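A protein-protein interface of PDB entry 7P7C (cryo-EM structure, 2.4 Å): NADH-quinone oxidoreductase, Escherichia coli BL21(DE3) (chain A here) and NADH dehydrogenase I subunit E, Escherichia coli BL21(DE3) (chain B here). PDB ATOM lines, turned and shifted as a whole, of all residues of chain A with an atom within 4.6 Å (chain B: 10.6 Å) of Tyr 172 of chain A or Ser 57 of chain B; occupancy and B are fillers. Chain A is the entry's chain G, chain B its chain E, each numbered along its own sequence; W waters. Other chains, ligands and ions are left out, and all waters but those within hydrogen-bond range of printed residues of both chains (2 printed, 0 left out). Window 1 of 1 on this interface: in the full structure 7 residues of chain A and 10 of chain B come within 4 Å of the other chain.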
ATOM      1  N   THR A 167       8.914  -7.856 -18.959  1.00  0.00           N
ATOM      2  CA  THR A 167       9.522  -6.829 -19.789  1.00  0.00           C
ATOM      3  C   THR A 167       8.631  -6.303 -20.905  1.00  0.00           C
ATOM      4  O   THR A 167       8.954  -5.257 -21.476  1.00  0.00           O
ATOM      5  CB  THR A 167      10.825  -7.349 -20.418  1.00  0.00           C
ATOM      6  OG1 THR A 167      10.560  -8.556 -21.143  1.00  0.00           O
ATOM      7  CG2 THR A 167      11.866  -7.624 -19.347  1.00  0.00           C
ATOM      8  N   ASP A 168       7.532  -6.976 -21.233  1.00  0.00           N
ATOM      9  CA  ASP A 168       6.735  -6.605 -22.393  1.00  0.00           C
ATOM     10  C   ASP A 168       5.484  -5.807 -22.042  1.00  0.00           C
ATOM     11  O   ASP A 168       4.622  -5.629 -22.904  1.00  0.00           O
ATOM     12  CB  ASP A 168       6.352  -7.849 -23.195  1.00  0.00           C
ATOM     13  CG  ASP A 168       5.661  -8.898 -22.357  1.00  0.00           C
ATOM     14  OD1 ASP A 168       6.019  -9.050 -21.174  1.00  0.00           O
ATOM     15  OD2 ASP A 168       4.759  -9.574 -22.885  1.00  0.00           O
ATOM     16  N   LEU A 169       5.361  -5.316 -20.815  1.00  0.00           N
ATOM     17  CA  LEU A 169       4.278  -4.416 -20.452  1.00  0.00           C
ATOM     18  C   LEU A 169       4.856  -3.077 -20.023  1.00  0.00           C
ATOM     19  O   LEU A 169       5.948  -3.007 -19.458  1.00  0.00           O
ATOM     20  CB  LEU A 169       3.408  -4.989 -19.334  1.00  0.00           C
ATOM     21  CG  LEU A 169       1.988  -4.440 -19.193  1.00  0.00           C
ATOM     22  CD1 LEU A 169       1.044  -5.148 -20.142  1.00  0.00           C
ATOM     23  CD2 LEU A 169       1.503  -4.565 -17.764  1.00  0.00           C
ATOM     24  N   GLY A 170       4.118  -2.014 -20.306  1.00  0.00           N
ATOM     25  CA  GLY A 170       4.598  -0.683 -20.004  1.00  0.00           C
ATOM     26  C   GLY A 170       3.500   0.339 -20.171  1.00  0.00           C
ATOM     27  O   GLY A 170       2.379   0.031 -20.594  1.00  0.00           O
ATOM     28  N   VAL A 171       3.845   1.573 -19.819  1.00  0.00           N
ATOM     29  CA  VAL A 171       2.963   2.721 -19.954  1.00  0.00           C
ATOM     30  C   VAL A 171       3.501   3.587 -21.086  1.00  0.00           C
ATOM     31  O   VAL A 171       4.712   3.807 -21.193  1.00  0.00           O
ATOM     32  CB  VAL A 171       2.842   3.498 -18.628  1.00  0.00           C
ATOM     33  CG1 VAL A 171       4.206   3.812 -18.036  1.00  0.00           C
ATOM     34  CG2 VAL A 171       2.008   4.759 -18.795  1.00  0.00           C
ATOM     35  N   TYR A 172       2.607   4.029 -21.960  1.00  0.00           N
ATOM     36  CA  TYR A 172       2.961   4.786 -23.144  1.00  0.00           C
ATOM     37  C   TYR A 172       2.109   6.039 -23.199  1.00  0.00           C
ATOM     38  O   TYR A 172       1.064   6.135 -22.553  1.00  0.00           O
ATOM     39  CB  TYR A 172       2.769   3.949 -24.414  1.00  0.00           C
ATOM     40  CG  TYR A 172       3.199   2.525 -24.219  1.00  0.00           C
ATOM     41  CD1 TYR A 172       4.544   2.190 -24.171  1.00  0.00           C
ATOM     42  CD2 TYR A 172       2.265   1.518 -24.040  1.00  0.00           C
ATOM     43  CE1 TYR A 172       4.946   0.894 -23.969  1.00  0.00           C
ATOM     44  CE2 TYR A 172       2.657   0.220 -23.841  1.00  0.00           C
ATOM     45  CZ  TYR A 172       3.998  -0.087 -23.805  1.00  0.00           C
ATOM     46  OH  TYR A 172       4.390  -1.384 -23.602  1.00  0.00           O
ATOM     47  N   GLY A 173       2.572   7.004 -23.968  1.00  0.00           N
ATOM     48  CA  GLY A 173       1.826   8.219 -24.151  1.00  0.00           C
ATOM     49  C   GLY A 173       2.037   9.210 -23.027  1.00  0.00           C
ATOM     50  O   GLY A 173       3.031   9.200 -22.298  1.00  0.00           O
ATOM     51  N   ALA A 174       1.045  10.073 -22.879  1.00  0.00           N
ATOM     52  CA  ALA A 174       1.180  11.299 -22.112  1.00  0.00           C
ATOM     53  C   ALA A 174      -0.175  11.602 -21.487  1.00  0.00           C
ATOM     54  O   ALA A 174      -1.043  10.730 -21.384  1.00  0.00           O
ATOM     55  CB  ALA A 174       1.714  12.436 -22.995  1.00  0.00           C
ATOM     56  N   ASN A 177      -3.834  10.645 -22.217  1.00  0.00           N
ATOM     57  CA  ASN A 177      -3.761   9.572 -23.193  1.00  0.00           C
ATOM     58  C   ASN A 177      -2.786   8.481 -22.767  1.00  0.00           C
ATOM     59  O   ASN A 177      -2.218   7.797 -23.623  1.00  0.00           O
ATOM     60  CB  ASN A 177      -3.367  10.141 -24.556  1.00  0.00           C
ATOM     61  CG  ASN A 177      -4.108   9.488 -25.695  1.00  0.00           C
ATOM     62  OD1 ASN A 177      -5.269   9.111 -25.560  1.00  0.00           O
ATOM     63  ND2 ASN A 177      -3.439   9.349 -26.830  1.00  0.00           N
ATOM     64  N   VAL A 178      -2.559   8.324 -21.460  1.00  0.00           N
ATOM     65  CA  VAL A 178      -1.684   7.263 -20.974  1.00  0.00           C
ATOM     66  C   VAL A 178      -2.311   5.910 -21.272  1.00  0.00           C
ATOM     67  O   VAL A 178      -3.495   5.675 -21.003  1.00  0.00           O
ATOM     68  CB  VAL A 178      -1.383   7.425 -19.475  1.00  0.00           C
ATOM     69  CG1 VAL A 178      -0.305   8.461 -19.256  1.00  0.00           C
ATOM     70  CG2 VAL A 178      -2.634   7.811 -18.709  1.00  0.00           C
ATOM     71  N   TYR A 179      -1.515   5.021 -21.846  1.00  0.00           N
ATOM     72  CA  TYR A 179      -1.973   3.735 -22.339  1.00  0.00           C
ATOM     73  C   TYR A 179      -1.131   2.652 -21.687  1.00  0.00           C
ATOM     74  O   TYR A 179       0.096   2.734 -21.694  1.00  0.00           O
ATOM     75  CB  TYR A 179      -1.846   3.685 -23.862  1.00  0.00           C
ATOM     76  CG  TYR A 179      -2.572   2.554 -24.532  1.00  0.00           C
ATOM     77  CD1 TYR A 179      -1.982   1.304 -24.666  1.00  0.00           C
ATOM     78  CD2 TYR A 179      -3.838   2.743 -25.061  1.00  0.00           C
ATOM     79  CE1 TYR A 179      -2.643   0.272 -25.293  1.00  0.00           C
ATOM     80  CE2 TYR A 179      -4.500   1.724 -25.687  1.00  0.00           C
ATOM     81  CZ  TYR A 179      -3.902   0.490 -25.801  1.00  0.00           C
ATOM     82  OH  TYR A 179      -4.571  -0.532 -26.427  1.00  0.00           O
ATOM     83  N   GLY A 181      -0.080  -1.277 -21.634  1.00  0.00           N
ATOM     84  CA  GLY A 181      -0.142  -2.477 -22.454  1.00  0.00           C
ATOM     85  C   GLY A 181       1.214  -2.864 -22.999  1.00  0.00           C
ATOM     86  O   GLY A 181       2.249  -2.543 -22.415  1.00  0.00           O
ATOM     87  N   ARG A 182       1.188  -3.565 -24.107  1.00  0.00           N
ATOM     88  CA  ARG A 182       2.373  -4.017 -24.812  1.00  0.00           C
ATOM     89  C   ARG A 182       2.713  -3.059 -25.943  1.00  0.00           C
ATOM     90  O   ARG A 182       1.852  -2.307 -26.405  1.00  0.00           O
ATOM     91  CB  ARG A 182       2.143  -5.426 -25.369  1.00  0.00           C
ATOM     92  CG  ARG A 182       1.863  -6.476 -24.322  1.00  0.00           C
ATOM     93  CD  ARG A 182       1.845  -7.857 -24.935  1.00  0.00           C
ATOM     94  NE  ARG A 182       3.172  -8.453 -25.016  1.00  0.00           N
ATOM     95  CZ  ARG A 182       3.844  -8.640 -26.144  1.00  0.00           C
ATOM     96  NH1 ARG A 182       3.357  -8.249 -27.309  1.00  0.00           N
ATOM     97  NH2 ARG A 182       5.030  -9.236 -26.102  1.00  0.00           N
ATOM     98  N   PRO A 183       3.972  -3.029 -26.398  1.00  0.00           N
ATOM     99  CA  PRO A 183       4.304  -2.184 -27.561  1.00  0.00           C
ATOM    100  C   PRO A 183       3.598  -2.594 -28.841  1.00  0.00           C
ATOM    101  O   PRO A 183       3.414  -1.750 -29.726  1.00  0.00           O
ATOM    102  CB  PRO A 183       5.828  -2.333 -27.686  1.00  0.00           C
ATOM    103  CG  PRO A 183       6.175  -3.535 -26.898  1.00  0.00           C
ATOM    104  CD  PRO A 183       5.178  -3.623 -25.798  1.00  0.00           C
ATOM    105  N   ARG B  23      20.766   3.004 -20.016  1.00  0.00           N
ATOM    106  CA  ARG B  23      19.380   3.423 -20.200  1.00  0.00           C
ATOM    107  C   ARG B  23      19.283   4.921 -20.461  1.00  0.00           C
ATOM    108  O   ARG B  23      18.386   5.372 -21.181  1.00  0.00           O
ATOM    109  CB  ARG B  23      18.556   3.036 -18.970  1.00  0.00           C
ATOM    110  CG  ARG B  23      17.096   3.458 -19.002  1.00  0.00           C
ATOM    111  CD  ARG B  23      16.441   3.276 -17.648  1.00  0.00           C
ATOM    112  NE  ARG B  23      16.346   1.870 -17.280  1.00  0.00           N
ATOM    113  CZ  ARG B  23      15.408   1.043 -17.719  1.00  0.00           C
ATOM    114  NH1 ARG B  23      14.450   1.454 -18.532  1.00  0.00           N
ATOM    115  NH2 ARG B  23      15.433  -0.229 -17.334  1.00  0.00           N
ATOM    116  N   SER B  26      18.690   6.535 -24.052  1.00  0.00           N
ATOM    117  CA  SER B  26      17.513   6.159 -24.833  1.00  0.00           C
ATOM    118  C   SER B  26      16.954   7.335 -25.625  1.00  0.00           C
ATOM    119  O   SER B  26      16.615   7.189 -26.807  1.00  0.00           O
ATOM    120  CB  SER B  26      16.440   5.576 -23.915  1.00  0.00           C
ATOM    121  OG  SER B  26      15.950   6.557 -23.021  1.00  0.00           O
ATOM    122  N   LEU B  30      16.904   7.621 -29.708  1.00  0.00           N
ATOM    123  CA  LEU B  30      15.694   7.911 -30.469  1.00  0.00           C
ATOM    124  C   LEU B  30      15.869   9.156 -31.327  1.00  0.00           C
ATOM    125  O   LEU B  30      15.419   9.190 -32.477  1.00  0.00           O
ATOM    126  CB  LEU B  30      14.505   8.074 -29.524  1.00  0.00           C
ATOM    127  CG  LEU B  30      13.961   6.799 -28.883  1.00  0.00           C
ATOM    128  CD1 LEU B  30      13.157   7.136 -27.647  1.00  0.00           C
ATOM    129  CD2 LEU B  30      13.118   6.021 -29.870  1.00  0.00           C
ATOM    130  N   ASP B  42       8.745   1.492 -36.353  1.00  0.00           N
ATOM    131  CA  ASP B  42       8.394   0.488 -35.349  1.00  0.00           C
ATOM    132  C   ASP B  42       9.575  -0.408 -34.989  1.00  0.00           C
ATOM    133  O   ASP B  42       9.768  -0.738 -33.814  1.00  0.00           O
ATOM    134  CB  ASP B  42       7.223  -0.358 -35.842  1.00  0.00           C
ATOM    135  CG  ASP B  42       5.952   0.446 -36.021  1.00  0.00           C
ATOM    136  OD1 ASP B  42       5.908   1.608 -35.572  1.00  0.00           O
ATOM    137  OD2 ASP B  42       4.990  -0.088 -36.613  1.00  0.00           O
ATOM    138  N   ALA B  44      12.690   0.351 -35.091  1.00  0.00           N
ATOM    139  CA  ALA B  44      13.723   1.115 -34.406  1.00  0.00           C
ATOM    140  C   ALA B  44      13.602   0.997 -32.895  1.00  0.00           C
ATOM    141  O   ALA B  44      14.614   1.080 -32.196  1.00  0.00           O
ATOM    142  CB  ALA B  44      13.663   2.581 -34.829  1.00  0.00           C
ATOM    143  N   ILE B  45      12.385   0.788 -32.384  1.00  0.00           N
ATOM    144  CA  ILE B  45      12.191   0.612 -30.946  1.00  0.00           C
ATOM    145  C   ILE B  45      12.921  -0.634 -30.463  1.00  0.00           C
ATOM    146  O   ILE B  45      13.693  -0.587 -29.498  1.00  0.00           O
ATOM    147  CB  ILE B  45      10.689   0.550 -30.612  1.00  0.00           C
ATOM    148  CG1 ILE B  45       9.991   1.843 -31.038  1.00  0.00           C
ATOM    149  CG2 ILE B  45      10.480   0.280 -29.131  1.00  0.00           C
ATOM    150  CD1 ILE B  45      10.585   3.092 -30.429  1.00  0.00           C
ATOM    151  N   HIS B  46      12.724  -1.758 -31.158  1.00  0.00           N
ATOM    152  CA  HIS B  46      13.405  -2.993 -30.784  1.00  0.00           C
ATOM    153  C   HIS B  46      14.903  -2.922 -31.045  1.00  0.00           C
ATOM    154  O   HIS B  46      15.686  -3.485 -30.271  1.00  0.00           O
ATOM    155  CB  HIS B  46      12.789  -4.179 -31.524  1.00  0.00           C
ATOM    156  CG  HIS B  46      11.493  -4.642 -30.938  1.00  0.00           C
ATOM    157  ND1 HIS B  46      10.280  -4.085 -31.282  1.00  0.00           N
ATOM    158  CD2 HIS B  46      11.220  -5.601 -30.022  1.00  0.00           C
ATOM    159  CE1 HIS B  46       9.316  -4.683 -30.607  1.00  0.00           C
ATOM    160  NE2 HIS B  46       9.860  -5.607 -29.836  1.00  0.00           N
ATOM    161  N   ALA B  47      15.322  -2.232 -32.111  1.00  0.00           N
ATOM    162  CA  ALA B  47      16.751  -2.090 -32.385  1.00  0.00           C
ATOM    163  C   ALA B  47      17.453  -1.287 -31.290  1.00  0.00           C
ATOM    164  O   ALA B  47      18.506  -1.693 -30.781  1.00  0.00           O
ATOM    165  CB  ALA B  47      16.954  -1.439 -33.751  1.00  0.00           C
ATOM    166  N   ILE B  48      16.867  -0.153 -30.899  1.00  0.00           N
ATOM    167  CA  ILE B  48      17.433   0.663 -29.829  1.00  0.00           C
ATOM    168  C   ILE B  48      17.404  -0.098 -28.511  1.00  0.00           C
ATOM    169  O   ILE B  48      18.361  -0.048 -27.725  1.00  0.00           O
ATOM    170  CB  ILE B  48      16.680   2.006 -29.744  1.00  0.00           C
ATOM    171  CG1 ILE B  48      17.060   2.905 -30.920  1.00  0.00           C
ATOM    172  CG2 ILE B  48      16.956   2.729 -28.441  1.00  0.00           C
ATOM    173  CD1 ILE B  48      16.112   4.056 -31.118  1.00  0.00           C
ATOM    174  N   ALA B  49      16.325  -0.850 -28.269  1.00  0.00           N
ATOM    175  CA  ALA B  49      16.210  -1.637 -27.047  1.00  0.00           C
ATOM    176  C   ALA B  49      17.294  -2.702 -26.953  1.00  0.00           C
ATOM    177  O   ALA B  49      17.889  -2.896 -25.888  1.00  0.00           O
ATOM    178  CB  ALA B  49      14.828  -2.280 -26.979  1.00  0.00           C
ATOM    179  N   ASP B  50      17.571  -3.404 -28.054  1.00  0.00           N
ATOM    180  CA  ASP B  50      18.582  -4.451 -27.986  1.00  0.00           C
ATOM    181  C   ASP B  50      19.994  -3.878 -27.962  1.00  0.00           C
ATOM    182  O   ASP B  50      20.908  -4.528 -27.443  1.00  0.00           O
ATOM    183  CB  ASP B  50      18.355  -5.485 -29.111  1.00  0.00           C
ATOM    184  CG  ASP B  50      18.670  -4.979 -30.532  1.00  0.00           C
ATOM    185  OD1 ASP B  50      17.972  -5.453 -31.453  1.00  0.00           O
ATOM    186  OD2 ASP B  50      19.633  -4.227 -30.790  1.00  0.00           O
ATOM    187  N   GLY B  53      20.206  -2.645 -24.151  1.00  0.00           N
ATOM    188  CA  GLY B  53      19.974  -3.618 -23.102  1.00  0.00           C
ATOM    189  C   GLY B  53      18.821  -3.282 -22.183  1.00  0.00           C
ATOM    190  O   GLY B  53      18.862  -3.623 -20.998  1.00  0.00           O
ATOM    191  N   ILE B  54      17.801  -2.612 -22.695  1.00  0.00           N
ATOM    192  CA  ILE B  54      16.592  -2.303 -21.936  1.00  0.00           C
ATOM    193  C   ILE B  54      15.419  -2.877 -22.717  1.00  0.00           C
ATOM    194  O   ILE B  54      15.538  -3.133 -23.926  1.00  0.00           O
ATOM    195  CB  ILE B  54      16.446  -0.784 -21.680  1.00  0.00           C
ATOM    196  CG1 ILE B  54      16.521   0.003 -22.986  1.00  0.00           C
ATOM    197  CG2 ILE B  54      17.500  -0.304 -20.700  1.00  0.00           C
ATOM    198  CD1 ILE B  54      16.278   1.478 -22.807  1.00  0.00           C
ATOM    199  N   PRO B  55      14.290  -3.148 -22.056  1.00  0.00           N
ATOM    200  CA  PRO B  55      13.130  -3.680 -22.781  1.00  0.00           C
ATOM    201  C   PRO B  55      12.573  -2.694 -23.794  1.00  0.00           C
ATOM    202  O   PRO B  55      12.709  -1.477 -23.657  1.00  0.00           O
ATOM    203  CB  PRO B  55      12.112  -3.955 -21.669  1.00  0.00           C
ATOM    204  CG  PRO B  55      12.918  -4.129 -20.453  1.00  0.00           C
ATOM    205  CD  PRO B  55      14.096  -3.224 -20.596  1.00  0.00           C
ATOM    206  N   ALA B  56      11.946  -3.246 -24.837  1.00  0.00           N
ATOM    207  CA  ALA B  56      11.325  -2.422 -25.867  1.00  0.00           C
ATOM    208  C   ALA B  56      10.134  -1.636 -25.342  1.00  0.00           C
ATOM    209  O   ALA B  56       9.808  -0.587 -25.906  1.00  0.00           O
ATOM    210  CB  ALA B  56      10.896  -3.288 -27.049  1.00  0.00           C
ATOM    211  N   SER B  57       9.480  -2.120 -24.285  1.00  0.00           N
ATOM    212  CA  SER B  57       8.395  -1.362 -23.672  1.00  0.00           C
ATOM    213  C   SER B  57       8.909  -0.063 -23.067  1.00  0.00           C
ATOM    214  O   SER B  57       8.238   0.970 -23.145  1.00  0.00           O
ATOM    215  CB  SER B  57       7.685  -2.211 -22.619  1.00  0.00           C
ATOM    216  OG  SER B  57       8.611  -2.855 -21.765  1.00  0.00           O
ATOM    217  N   ASP B  58      10.110  -0.091 -22.480  1.00  0.00           N
ATOM    218  CA  ASP B  58      10.716   1.127 -21.948  1.00  0.00           C
ATOM    219  C   ASP B  58      11.023   2.129 -23.056  1.00  0.00           C
ATOM    220  O   ASP B  58      10.748   3.328 -22.913  1.00  0.00           O
ATOM    221  CB  ASP B  58      11.991   0.779 -21.180  1.00  0.00           C
ATOM    222  CG  ASP B  58      11.708   0.139 -19.837  1.00  0.00           C
ATOM    223  OD1 ASP B  58      12.635  -0.461 -19.256  1.00  0.00           O
ATOM    224  OD2 ASP B  58      10.560   0.236 -19.357  1.00  0.00           O
ATOM    225  N   VAL B  59      11.577   1.647 -24.172  1.00  0.00           N
ATOM    226  CA  VAL B  59      11.903   2.516 -25.298  1.00  0.00           C
ATOM    227  C   VAL B  59      10.639   3.112 -25.901  1.00  0.00           C
ATOM    228  O   VAL B  59      10.599   4.300 -26.238  1.00  0.00           O
ATOM    229  CB  VAL B  59      12.723   1.739 -26.345  1.00  0.00           C
ATOM    230  CG1 VAL B  59      13.077   2.628 -27.526  1.00  0.00           C
ATOM    231  CG2 VAL B  59      13.976   1.171 -25.714  1.00  0.00           C
ATOM    232  N   GLU B  60       9.580   2.309 -26.023  1.00  0.00           N
ATOM    233  CA  GLU B  60       8.334   2.819 -26.587  1.00  0.00           C
ATOM    234  C   GLU B  60       7.646   3.795 -25.637  1.00  0.00           C
ATOM    235  O   GLU B  60       7.049   4.780 -26.085  1.00  0.00           O
ATOM    236  CB  GLU B  60       7.409   1.657 -26.954  1.00  0.00           C
ATOM    237  CG  GLU B  60       6.028   2.060 -27.475  1.00  0.00           C
ATOM    238  CD  GLU B  60       6.013   2.461 -28.946  1.00  0.00           C
ATOM    239  OE1 GLU B  60       7.082   2.739 -29.523  1.00  0.00           O
ATOM    240  OE2 GLU B  60       4.912   2.499 -29.533  1.00  0.00           O
ATOM    241  N   GLY B  61       7.732   3.554 -24.327  1.00  0.00           N
ATOM    242  CA  GLY B  61       7.183   4.503 -23.372  1.00  0.00           C
ATOM    243  C   GLY B  61       7.903   5.836 -23.402  1.00  0.00           C
ATOM    244  O   GLY B  61       7.271   6.894 -23.321  1.00  0.00           O
ATOM    245  N   VAL B  62       9.229   5.802 -23.546  1.00  0.00           N
ATOM    246  CA  VAL B  62       9.994   7.036 -23.704  1.00  0.00           C
ATOM    247  C   VAL B  62       9.614   7.737 -25.005  1.00  0.00           C
ATOM    248  O   VAL B  62       9.345   8.942 -25.021  1.00  0.00           O
ATOM    249  CB  VAL B  62      11.504   6.743 -23.634  1.00  0.00           C
ATOM    250  CG1 VAL B  62      12.305   7.937 -24.103  1.00  0.00           C
ATOM    251  CG2 VAL B  62      11.899   6.368 -22.219  1.00  0.00           C
ATOM    252  N   ALA B  63       9.545   6.982 -26.107  1.00  0.00           N
ATOM    253  CA  ALA B  63       9.286   7.576 -27.418  1.00  0.00           C
ATOM    254  C   ALA B  63       7.898   8.197 -27.497  1.00  0.00           C
ATOM    255  O   ALA B  63       7.726   9.264 -28.095  1.00  0.00           O
ATOM    256  CB  ALA B  63       9.462   6.525 -28.511  1.00  0.00           C
ATOM    257  N   THR B  64       6.896   7.552 -26.901  1.00  0.00           N
ATOM    258  CA  THR B  64       5.551   8.104 -26.910  1.00  0.00           C
ATOM    259  C   THR B  64       5.329   9.142 -25.820  1.00  0.00           C
ATOM    260  O   THR B  64       4.335   9.869 -25.878  1.00  0.00           O
ATOM    261  CB  THR B  64       4.518   6.986 -26.767  1.00  0.00           C
ATOM    262  OG1 THR B  64       4.816   6.209 -25.604  1.00  0.00           O
ATOM    263  CG2 THR B  64       4.537   6.088 -27.989  1.00  0.00           C
ATOM    264  N   PHE B  65       6.215   9.224 -24.823  1.00  0.00           N
ATOM    265  CA  PHE B  65       6.089  10.292 -23.838  1.00  0.00           C
ATOM    266  C   PHE B  65       6.498  11.642 -24.418  1.00  0.00           C
ATOM    267  O   PHE B  65       5.820  12.650 -24.191  1.00  0.00           O
ATOM    268  CB  PHE B  65       6.921   9.975 -22.597  1.00  0.00           C
ATOM    269  CG  PHE B  65       6.751  10.968 -21.484  1.00  0.00           C
ATOM    270  CD1 PHE B  65       5.687  10.864 -20.607  1.00  0.00           C
ATOM    271  CD2 PHE B  65       7.655  12.004 -21.311  1.00  0.00           C
ATOM    272  CE1 PHE B  65       5.524  11.775 -19.583  1.00  0.00           C
ATOM    273  CE2 PHE B  65       7.494  12.917 -20.294  1.00  0.00           C
ATOM    274  CZ  PHE B  65       6.430  12.801 -19.427  1.00  0.00           C
ATOM    275  N   TYR B  66       7.598  11.685 -25.159  1.00  0.00           N
ATOM    276  CA  TYR B  66       8.180  12.947 -25.595  1.00  0.00           C
ATOM    277  C   TYR B  66       7.612  13.353 -26.947  1.00  0.00           C
ATOM    278  O   TYR B  66       7.581  12.552 -27.885  1.00  0.00           O
ATOM    279  CB  TYR B  66       9.701  12.835 -25.653  1.00  0.00           C
ATOM    280  CG  TYR B  66      10.313  12.662 -24.285  1.00  0.00           C
ATOM    281  CD1 TYR B  66      10.454  13.738 -23.425  1.00  0.00           C
ATOM    282  CD2 TYR B  66      10.725  11.417 -23.842  1.00  0.00           C
ATOM    283  CE1 TYR B  66      10.997  13.576 -22.174  1.00  0.00           C
ATOM    284  CE2 TYR B  66      11.267  11.245 -22.595  1.00  0.00           C
ATOM    285  CZ  TYR B  66      11.403  12.328 -21.764  1.00  0.00           C
ATOM    286  OH  TYR B  66      11.947  12.160 -20.516  1.00  0.00           O
ATOM    287  N   ARG B  71       6.642   9.186 -33.776  1.00  0.00           N
ATOM    288  CA  ARG B  71       6.366   7.772 -33.974  1.00  0.00           C
ATOM    289  C   ARG B  71       5.386   7.536 -35.115  1.00  0.00           C
ATOM    290  O   ARG B  71       4.907   6.412 -35.292  1.00  0.00           O
ATOM    291  CB  ARG B  71       5.847   7.155 -32.677  1.00  0.00           C
ATOM    292  CG  ARG B  71       6.938   6.806 -31.688  1.00  0.00           C
ATOM    293  CD  ARG B  71       7.828   5.717 -32.235  1.00  0.00           C
ATOM    294  NE  ARG B  71       7.255   4.401 -31.990  1.00  0.00           N
ATOM    295  CZ  ARG B  71       6.851   3.571 -32.940  1.00  0.00           C
ATOM    296  NH1 ARG B  71       6.951   3.884 -34.221  1.00  0.00           N
ATOM    297  NH2 ARG B  71       6.331   2.397 -32.597  1.00  0.00           N
HETATM  298  O   HOH W   1      10.018  -3.636 -18.936  1.00  0.00           O
HETATM  299  O   HOH W   2       9.324  -5.099 -23.964  1.00  0.00           O
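OG of Ser 57 of chain B sits at hydrogen-bond distance from O of Thr 167 of chain A, 2.4 Å away.
The backbone NH of Gly 173 of chain A is in hydrogen-bond range of the side-chain hydroxyl of Thr 64 of chain B, 2.9 Å away.
Of chain B, only Ser 57, Glu 60, Gly 61 and Thr 64 come within 4 Å of Tyr 172 of chain A.
Of chain A, only Thr 167, Leu 169 and Tyr 172 come within 4 Å of Ser 57 of chain B.
Thr 167 of chain A touches just these residues of chain B: Pro 55 (3.4 Å) and Ser 57 (2.4 Å).
No residue of chain B comes within 4 Å of Gly 170 of chain A.
Val 171 of chain A touches one residue of chain B.
Gly 173 of chain A touches two residues of chain B.
No residue of chain B comes within 4 Å of Val 178 of chain A.
No residue of chain B comes within 4 Å of Gly 181 of chain A.
No residue of chain B comes within 4 Å of Pro 183 of chain A.
Of the printed residues of chain A, Glu 60 of chain B touches Tyr 172.
Of the printed residues of chain A, Thr 64 of chain B touches Tyr 172 and Gly 173.
Of the printed residues of chain A, Gly 61 of chain B touches Val 171 and Tyr 172.
Printed residues of chain A within 4 Å of Pro 55 of chain B: Thr 167 (3.4 Å).
Val 59 of chain B touches none of the printed residues of chain A.
The nearest printed residue of chain A that does not touch Thr 64 of chain B is Ala 174 of chain A (4.5 Å).
O of Thr 167 of chain A touches CB of Pro 55 of chain B, at 3.4 Å.
Leu 169 of chain A touches Ser 57 of chain B (O to OG, 3.5 Å).
O of Val 171 of chain A touches CA of Gly 61 of chain B, at 3.4 Å.
Ser 57 of chain B touches Tyr 172 of chain A (O to CE1, 3.4 Å).
Tyr 172 of chain A touches Glu 60 of chain B (CD1 to CG, 3.6 Å).
Gly 61 of chain B touches Tyr 172 of chain A (N to CD1, 3.5 Å).
CB of Tyr 172 of chain A touches OG1 of Thr 64 of chain B, at 3.3 Å.
O of Gly 173 of chain A touches CD1 of Phe 65 of chain B, 3.6 Å away.
The backbone carbonyl oxygen (O) of Glu 60 of chain B lies within hydrogen-bond range of the side-chain hydroxyl (OG1) of Thr 64 of chain B.
NE of Arg 71 of chain B lies within salt-bridge range of OE1 of Glu 60 of chain B (3.0 Å).
OG1 of Thr 64 of chain B sits at hydrogen-bond distance from O of Gly 61 of chain B (3.4 Å).
The side-chain hydroxyl (OH) of Tyr 172 of chain A is in hydrogen-bond range of the backbone NH (N) of Gly 170 of chain A, 3.4 Å away.
N of Tyr 172 of chain A is in hydrogen-bond range of O of Tyr 179 of chain A (2.8 Å).
The side-chain hydroxyl of Tyr 172 of chain A lies within hydrogen-bond range of the backbone carbonyl oxygen of Gly 181 of chain A.
Of the 14 printed residues of chain A, 5 touch a printed residue of chain B.
Hydrophobic or aromatic side chains of chain A that line the printed part of chain B: Tyr 172.
Of the 26 printed residues of chain B, 6 touch a printed residue of chain A.
Among the printed residues, no Asp or Glu carboxylate lies within 4 Å of a Lys or Arg side-chain nitrogen of the other chain.
Water W2 lies within hydrogen-bond range of the backbone carbonyl oxygen of Thr 167 of chain A (2.5 Å), the backbone NH of Ser 57 of chain B (3.0 Å) and the backbone NH of Ala 56 of chain B (3.3 Å).
Water W1 bridges the backbone carbonyl oxygen (O) of Thr 167 of chain A (3.2 Å) and the side-chain hydroxyl (OG) of Ser 57 of chain B (3.3 Å).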
